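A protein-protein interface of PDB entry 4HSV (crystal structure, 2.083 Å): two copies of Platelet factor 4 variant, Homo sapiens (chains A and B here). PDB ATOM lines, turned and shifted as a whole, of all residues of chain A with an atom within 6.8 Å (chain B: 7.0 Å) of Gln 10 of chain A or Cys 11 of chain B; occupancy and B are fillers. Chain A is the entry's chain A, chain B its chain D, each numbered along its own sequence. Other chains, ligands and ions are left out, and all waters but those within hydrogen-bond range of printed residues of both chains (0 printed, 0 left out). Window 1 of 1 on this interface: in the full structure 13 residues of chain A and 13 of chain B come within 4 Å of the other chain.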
ATOM      1  N   GLY A   7     -17.842  -7.530   9.499  1.00  0.00           N
ATOM      2  CA  GLY A   7     -19.219  -7.300   9.902  1.00  0.00           C
ATOM      3  C   GLY A   7     -20.151  -7.192   8.709  1.00  0.00           C
ATOM      4  O   GLY A   7     -19.705  -7.343   7.560  1.00  0.00           O
ATOM      5  N   ASP A   8     -21.436  -6.950   8.989  1.00  0.00           N
ATOM      6  CA  ASP A   8     -22.465  -6.829   7.958  1.00  0.00           C
ATOM      7  C   ASP A   8     -22.318  -5.566   7.122  1.00  0.00           C
ATOM      8  O   ASP A   8     -22.772  -5.539   5.986  1.00  0.00           O
ATOM      9  CB  ASP A   8     -23.877  -6.797   8.569  1.00  0.00           C
ATOM     10  CG  ASP A   8     -24.391  -8.162   8.992  1.00  0.00           C
ATOM     11  OD1 ASP A   8     -23.668  -8.858   9.751  1.00  0.00           O
ATOM     12  OD2 ASP A   8     -25.556  -8.496   8.589  1.00  0.00           O
ATOM     13  N   LEU A   9     -21.715  -4.528   7.699  1.00  0.00           N
ATOM     14  CA  LEU A   9     -21.670  -3.192   7.078  1.00  0.00           C
ATOM     15  C   LEU A   9     -20.253  -2.791   6.699  1.00  0.00           C
ATOM     16  O   LEU A   9     -19.284  -3.289   7.283  1.00  0.00           O
ATOM     17  CB  LEU A   9     -22.206  -2.148   8.068  1.00  0.00           C
ATOM     18  CG  LEU A   9     -23.720  -1.987   8.298  1.00  0.00           C
ATOM     19  CD1 LEU A   9     -24.320  -3.233   8.860  1.00  0.00           C
ATOM     20  CD2 LEU A   9     -23.957  -0.831   9.275  1.00  0.00           C
ATOM     21  N   GLN A  10     -20.128  -1.882   5.733  1.00  0.00           N
ATOM     22  CA  GLN A  10     -18.821  -1.351   5.374  1.00  0.00           C
ATOM     23  C   GLN A  10     -18.845   0.172   5.448  1.00  0.00           C
ATOM     24  O   GLN A  10     -19.848   0.772   5.862  1.00  0.00           O
ATOM     25  CB  GLN A  10     -18.413  -1.828   3.977  1.00  0.00           C
ATOM     26  CG  GLN A  10     -19.448  -1.490   2.904  1.00  0.00           C
ATOM     27  CD  GLN A  10     -19.048  -1.942   1.516  1.00  0.00           C
ATOM     28  OE1 GLN A  10     -17.957  -2.471   1.312  1.00  0.00           O
ATOM     29  NE2 GLN A  10     -19.953  -1.777   0.555  1.00  0.00           N
ATOM     30  N   CYS A  11     -17.747   0.800   5.041  1.00  0.00           N
ATOM     31  CA  CYS A  11     -17.655   2.262   5.020  1.00  0.00           C
ATOM     32  C   CYS A  11     -18.598   2.802   3.941  1.00  0.00           C
ATOM     33  O   CYS A  11     -18.569   2.326   2.795  1.00  0.00           O
ATOM     34  CB  CYS A  11     -16.209   2.690   4.719  1.00  0.00           C
ATOM     35  SG  CYS A  11     -15.028   2.319   6.022  1.00  0.00           S
ATOM     36  N   LEU A  12     -19.475   3.723   4.310  1.00  0.00           N
ATOM     37  CA  LEU A  12     -20.381   4.361   3.345  1.00  0.00           C
ATOM     38  C   LEU A  12     -19.607   5.200   2.296  1.00  0.00           C
ATOM     39  O   LEU A  12     -19.941   5.230   1.105  1.00  0.00           O
ATOM     40  CB  LEU A  12     -21.358   5.277   4.087  1.00  0.00           C
ATOM     41  CG  LEU A  12     -22.559   5.713   3.264  1.00  0.00           C
ATOM     42  CD1 LEU A  12     -23.466   4.509   3.079  1.00  0.00           C
ATOM     43  CD2 LEU A  12     -23.309   6.855   3.944  1.00  0.00           C
ATOM     44  N   CYS A  13     -18.554   5.870   2.749  1.00  0.00           N
ATOM     45  CA  CYS A  13     -17.831   6.812   1.900  1.00  0.00           C
ATOM     46  C   CYS A  13     -16.758   6.144   1.082  1.00  0.00           C
ATOM     47  O   CYS A  13     -15.868   5.519   1.653  1.00  0.00           O
ATOM     48  CB  CYS A  13     -17.157   7.860   2.776  1.00  0.00           C
ATOM     49  SG  CYS A  13     -18.340   8.928   3.635  1.00  0.00           S
ATOM     50  N   VAL A  14     -16.828   6.304  -0.242  1.00  0.00           N
ATOM     51  CA  VAL A  14     -15.782   5.863  -1.156  1.00  0.00           C
ATOM     52  C   VAL A  14     -14.855   7.025  -1.555  1.00  0.00           C
ATOM     53  O   VAL A  14     -13.635   6.863  -1.694  1.00  0.00           O
ATOM     54  CB  VAL A  14     -16.384   5.238  -2.446  1.00  0.00           C
ATOM     55  CG1 VAL A  14     -15.279   4.805  -3.427  1.00  0.00           C
ATOM     56  CG2 VAL A  14     -17.239   4.057  -2.093  1.00  0.00           C
ATOM     57  N   PRO A  35     -17.354  -1.037  14.012  1.00  0.00           N
ATOM     58  CA  PRO A  35     -17.252  -2.340  13.347  1.00  0.00           C
ATOM     59  C   PRO A  35     -17.456  -2.187  11.844  1.00  0.00           C
ATOM     60  O   PRO A  35     -16.877  -2.915  11.039  1.00  0.00           O
ATOM     61  CB  PRO A  35     -18.422  -3.133  13.958  1.00  0.00           C
ATOM     62  CG  PRO A  35     -18.669  -2.480  15.287  1.00  0.00           C
ATOM     63  CD  PRO A  35     -18.398  -1.025  15.055  1.00  0.00           C
ATOM     64  N   HIS A  36     -18.265  -1.208  11.471  1.00  0.00           N
ATOM     65  CA  HIS A  36     -18.633  -0.993  10.082  1.00  0.00           C
ATOM     66  C   HIS A  36     -17.547  -0.277   9.271  1.00  0.00           C
ATOM     67  O   HIS A  36     -17.476  -0.446   8.060  1.00  0.00           O
ATOM     68  CB  HIS A  36     -19.886  -0.124  10.054  1.00  0.00           C
ATOM     69  CG  HIS A  36     -19.674   1.194  10.726  1.00  0.00           C
ATOM     70  ND1 HIS A  36     -19.585   1.319  12.094  1.00  0.00           N
ATOM     71  CD2 HIS A  36     -19.421   2.426  10.212  1.00  0.00           C
ATOM     72  CE1 HIS A  36     -19.341   2.584  12.401  1.00  0.00           C
ATOM     73  NE2 HIS A  36     -19.237   3.273  11.277  1.00  0.00           N
ATOM     74  N   CYS A  37     -16.734   0.542   9.938  1.00  0.00           N
ATOM     75  CA  CYS A  37     -15.739   1.379   9.256  1.00  0.00           C
ATOM     76  C   CYS A  37     -14.676   1.832  10.231  1.00  0.00           C
ATOM     77  O   CYS A  37     -15.010   2.402  11.265  1.00  0.00           O
ATOM     78  CB  CYS A  37     -16.411   2.618   8.655  1.00  0.00           C
ATOM     79  SG  CYS A  37     -15.353   3.607   7.581  1.00  0.00           S
ATOM     80  N   GLN A  41     -16.664   9.032   9.491  1.00  0.00           N
ATOM     81  CA  GLN A  41     -17.104   9.546   8.191  1.00  0.00           C
ATOM     82  C   GLN A  41     -17.967  10.803   8.389  1.00  0.00           C
ATOM     83  O   GLN A  41     -18.732  10.885   9.337  1.00  0.00           O
ATOM     84  CB  GLN A  41     -17.889   8.472   7.410  1.00  0.00           C
ATOM     85  CG  GLN A  41     -17.128   7.168   7.134  1.00  0.00           C
ATOM     86  CD  GLN A  41     -18.059   6.093   6.600  1.00  0.00           C
ATOM     87  OE1 GLN A  41     -18.227   5.935   5.383  1.00  0.00           O
ATOM     88  NE2 GLN A  41     -18.724   5.386   7.526  1.00  0.00           N
ATOM     89  N   LEU B   9     -20.424   7.625  -2.696  1.00  0.00           N
ATOM     90  CA  LEU B   9     -20.852   6.732  -1.615  1.00  0.00           C
ATOM     91  C   LEU B   9     -21.072   5.347  -2.183  1.00  0.00           C
ATOM     92  O   LEU B   9     -21.231   5.203  -3.397  1.00  0.00           O
ATOM     93  CB  LEU B   9     -22.154   7.220  -0.956  1.00  0.00           C
ATOM     94  CG  LEU B   9     -22.094   8.338   0.098  1.00  0.00           C
ATOM     95  CD1 LEU B   9     -21.615   9.608  -0.511  1.00  0.00           C
ATOM     96  CD2 LEU B   9     -23.478   8.559   0.731  1.00  0.00           C
ATOM     97  N   GLN B  10     -21.063   4.332  -1.325  1.00  0.00           N
ATOM     98  CA  GLN B  10     -21.409   2.991  -1.769  1.00  0.00           C
ATOM     99  C   GLN B  10     -22.492   2.376  -0.900  1.00  0.00           C
ATOM    100  O   GLN B  10     -23.029   3.028  -0.007  1.00  0.00           O
ATOM    101  CB  GLN B  10     -20.176   2.081  -1.771  1.00  0.00           C
ATOM    102  CG  GLN B  10     -19.471   1.999  -0.414  1.00  0.00           C
ATOM    103  CD  GLN B  10     -18.242   1.085  -0.452  1.00  0.00           C
ATOM    104  OE1 GLN B  10     -17.937   0.488  -1.484  1.00  0.00           O
ATOM    105  NE2 GLN B  10     -17.505   1.025   0.654  1.00  0.00           N
ATOM    106  N   CYS B  11     -22.765   1.097  -1.139  1.00  0.00           N
ATOM    107  CA  CYS B  11     -23.755   0.344  -0.379  1.00  0.00           C
ATOM    108  C   CYS B  11     -23.245   0.136   1.045  1.00  0.00           C
ATOM    109  O   CYS B  11     -22.121  -0.325   1.240  1.00  0.00           O
ATOM    110  CB  CYS B  11     -24.026  -1.023  -1.053  1.00  0.00           C
ATOM    111  SG  CYS B  11     -24.882  -0.953  -2.650  1.00  0.00           S
ATOM    112  N   LEU B  12     -24.046   0.508   2.035  1.00  0.00           N
ATOM    113  CA  LEU B  12     -23.668   0.289   3.427  1.00  0.00           C
ATOM    114  C   LEU B  12     -23.560  -1.204   3.756  1.00  0.00           C
ATOM    115  O   LEU B  12     -22.693  -1.628   4.521  1.00  0.00           O
ATOM    116  CB  LEU B  12     -24.691   0.911   4.366  1.00  0.00           C
ATOM    117  CG  LEU B  12     -24.223   0.997   5.809  1.00  0.00           C
ATOM    118  CD1 LEU B  12     -23.092   2.018   5.906  1.00  0.00           C
ATOM    119  CD2 LEU B  12     -25.386   1.370   6.713  1.00  0.00           C
ATOM    120  N   CYS B  13     -24.455  -1.995   3.177  1.00  0.00           N
ATOM    121  CA  CYS B  13     -24.575  -3.412   3.533  1.00  0.00           C
ATOM    122  C   CYS B  13     -23.683  -4.319   2.706  1.00  0.00           C
ATOM    123  O   CYS B  13     -23.798  -4.368   1.494  1.00  0.00           O
ATOM    124  CB  CYS B  13     -26.014  -3.857   3.350  1.00  0.00           C
ATOM    125  SG  CYS B  13     -27.176  -3.033   4.516  1.00  0.00           S
ATOM    126  N   VAL B  14     -22.848  -5.075   3.397  1.00  0.00           N
ATOM    127  CA  VAL B  14     -21.997  -6.088   2.783  1.00  0.00           C
ATOM    128  C   VAL B  14     -22.651  -7.447   2.923  1.00  0.00           C
ATOM    129  O   VAL B  14     -22.565  -8.283   2.025  1.00  0.00           O
ATOM    130  CB  VAL B  14     -20.621  -6.096   3.439  1.00  0.00           C
ATOM    131  CG1 VAL B  14     -19.753  -7.287   2.961  1.00  0.00           C
ATOM    132  CG2 VAL B  14     -19.926  -4.814   3.091  1.00  0.00           C
ATOM    133  N   LYS B  15     -23.251  -7.686   4.082  1.00  0.00           N
ATOM    134  CA  LYS B  15     -23.941  -8.944   4.343  1.00  0.00           C
ATOM    135  C   LYS B  15     -25.403  -8.702   4.639  1.00  0.00           C
ATOM    136  O   LYS B  15     -25.745  -7.663   5.192  1.00  0.00           O
ATOM    137  CB  LYS B  15     -23.316  -9.646   5.548  1.00  0.00           C
ATOM    138  CG  LYS B  15     -21.911 -10.170   5.359  1.00  0.00           C
ATOM    139  CD  LYS B  15     -21.404 -10.787   6.689  1.00  0.00           C
ATOM    140  CE  LYS B  15     -19.902 -11.029   6.673  1.00  0.00           C
ATOM    141  NZ  LYS B  15     -19.587 -12.212   5.836  1.00  0.00           N
ATOM    142  N   HIS B  36     -25.701   6.007  -4.580  1.00  0.00           N
ATOM    143  CA  HIS B  36     -24.841   5.313  -3.636  1.00  0.00           C
ATOM    144  C   HIS B  36     -24.997   3.794  -3.712  1.00  0.00           C
ATOM    145  O   HIS B  36     -24.088   3.060  -3.366  1.00  0.00           O
ATOM    146  CB  HIS B  36     -25.209   5.762  -2.225  1.00  0.00           C
ATOM    147  CG  HIS B  36     -26.632   5.462  -1.887  1.00  0.00           C
ATOM    148  ND1 HIS B  36     -27.676   6.266  -2.295  1.00  0.00           N
ATOM    149  CD2 HIS B  36     -27.199   4.403  -1.258  1.00  0.00           C
ATOM    150  CE1 HIS B  36     -28.819   5.733  -1.906  1.00  0.00           C
ATOM    151  NE2 HIS B  36     -28.558   4.600  -1.273  1.00  0.00           N
ATOM    152  N   CYS B  37     -26.165   3.322  -4.130  1.00  0.00           N
ATOM    153  CA  CYS B  37     -26.430   1.884  -4.124  1.00  0.00           C
ATOM    154  C   CYS B  37     -27.589   1.565  -5.035  1.00  0.00           C
ATOM    155  O   CYS B  37     -28.645   2.201  -4.935  1.00  0.00           O
ATOM    156  CB  CYS B  37     -26.743   1.417  -2.695  1.00  0.00           C
ATOM    157  SG  CYS B  37     -26.855  -0.407  -2.433  1.00  0.00           S
ATOM    158  N   PRO B  38     -27.401   0.595  -5.945  1.00  0.00           N
ATOM    159  CA  PRO B  38     -28.471   0.307  -6.899  1.00  0.00           C
ATOM    160  C   PRO B  38     -29.659  -0.401  -6.247  1.00  0.00           C
ATOM    161  O   PRO B  38     -30.705  -0.505  -6.879  1.00  0.00           O
ATOM    162  CB  PRO B  38     -27.776  -0.592  -7.939  1.00  0.00           C
ATOM    163  CG  PRO B  38     -26.685  -1.279  -7.166  1.00  0.00           C
ATOM    164  CD  PRO B  38     -26.199  -0.225  -6.192  1.00  0.00           C
ATOM    165  N   THR B  39     -29.500  -0.905  -5.024  1.00  0.00           N
ATOM    166  CA  THR B  39     -30.619  -1.545  -4.314  1.00  0.00           C
ATOM    167  C   THR B  39     -30.975  -0.891  -2.963  1.00  0.00           C
ATOM    168  O   THR B  39     -30.120  -0.268  -2.317  1.00  0.00           O
ATOM    169  CB  THR B  39     -30.342  -3.063  -4.101  1.00  0.00           C
ATOM    170  OG1 THR B  39     -31.489  -3.683  -3.518  1.00  0.00           O
ATOM    171  CG2 THR B  39     -29.139  -3.292  -3.190  1.00  0.00           C
ATOM    172  N   GLN B  41     -31.702  -0.868   0.952  1.00  0.00           N
ATOM    173  CA  GLN B  41     -31.079  -1.639   2.040  1.00  0.00           C
ATOM    174  C   GLN B  41     -31.913  -1.473   3.308  1.00  0.00           C
ATOM    175  O   GLN B  41     -32.458  -0.406   3.547  1.00  0.00           O
ATOM    176  CB  GLN B  41     -29.648  -1.153   2.284  1.00  0.00           C
ATOM    177  CG  GLN B  41     -28.717  -1.198   1.058  1.00  0.00           C
ATOM    178  CD  GLN B  41     -27.450  -0.425   1.320  1.00  0.00           C
ATOM    179  OE1 GLN B  41     -26.457  -0.992   1.789  1.00  0.00           O
ATOM    180  NE2 GLN B  41     -27.486   0.908   1.064  1.00  0.00           N
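Of the 12 printed residues of chain B, 7 touch a printed residue of chain A.
Hydrophobic or aromatic side chains of chain B that line the printed part of chain A: Leu 9, Leu 12 and Val 14.
Of the 12 printed residues of chain A, 7 touch a printed residue of chain B.
Hydrophobic or aromatic side chains of chain A that line the printed part of chain B: Leu 9, Leu 12 and Val 14.
Gln 10 of chain B touches its own counterpart, Gln 10 of chain A.
Gln 10 of chain A touches Cys 11 of chain B, and with the chains exchanged Cys 11 of chain A touches Gln 10 of chain B.
Gln 10 of chain A touches Leu 12 of chain B, and with the chains exchanged Leu 12 of chain A touches Gln 10 of chain B.
Leu 12 of chain B touches its own counterpart, Leu 12 of chain A.
Positions printed for both chains: 9, 10, 11, 12, 13, 14, 36, 37 and 41.
Of the 14 pairs that touch across the chains among the printed residues, 10 have their exchanged pair printed and touching as well.
Gln 10 of chain A touches four residues of chain B.
Of chain A, only Gln 10 comes within 4 Å of Cys 11 of chain B.
Printed residues of chain A within 4 Å of Cys 13 of chain B: Asp 8.
Of the printed residues of chain B, Cys 11 of chain A touches Gln 10.
Of the printed residues of chain A, Lys 15 of chain B touches Gly 7 and Asp 8.
Printed residues of chain B within 4 Å of Gly 7 of chain A: Lys 15 (3.8 Å).
The nearest residue of chain B that does not touch Gln 10 of chain A is Cys 13 of chain B (4.7 Å).
The nearest printed residue of chain A that does not touch Gln 10 of chain B is Cys 13 of chain A (4.9 Å).
The backbone carbonyl oxygen (O) of His 36 of chain A sits at hydrogen-bond distance from the backbone NH (N) of Cys 11 of chain A (3.3 Å).
SG of Cys 11 of chain A is disulfide-bonded to SG of Cys 37 of chain A (2.0 Å).
O of His 36 of chain B lies within hydrogen-bond range of N of Cys 11 of chain B (3.3 Å).
SG of Cys 11 of chain B is disulfide-bonded to SG of Cys 37 of chain B, 2.1 Å away.
OE1 of Gln 41 of chain B sits at hydrogen-bond distance from N of Leu 12 of chain B, 2.9 Å away.
N of Cys 13 of chain B is in hydrogen-bond range of OE1 of Gln 41 of chain B (2.6 Å).
Gly 7 of chain A touches Lys 15 of chain B.
Asp 8 of chain A touches Cys 13 of chain B (O to C, 3.6 Å).
CA of Leu 9 of chain A touches O of Leu 12 of chain B, 3.2 Å away.
Gln 10 of chain A touches Gln 10 of chain B.
Val 14 of chain B touches Gln 10 of chain A (CG2 to CG, 3.4 Å).
CA of Leu 9 of chain B touches O of Leu 12 of chain A, at 3.2 Å.
CD1 of Leu 12 of chain A touches CD1 of Leu 12 of chain B (3.8 Å).
Gln 10 of chain B touches Val 14 of chain A (CG to CG2, 3.5 Å).
The backbone carbonyl oxygen (O) of Asp 8 of chain A sits at hydrogen-bond distance from the backbone NH (N) of Val 14 of chain B (2.6 Å).
O of Asp 8 of chain A is in hydrogen-bond range of N of Lys 15 of chain B, 2.9 Å away.
O of Cys 11 of chain B is in hydrogen-bond range of NE2 of Gln 10 of chain A, 2.7 Å away.
N of Gln 10 of chain A sits at hydrogen-bond distance from O of Leu 12 of chain B, at 2.8 Å.
O of Cys 11 of chain A is in hydrogen-bond range of NE2 of Gln 10 of chain B.
N of Gln 10 of chain B sits at hydrogen-bond distance from O of Leu 12 of chain A (2.8 Å).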
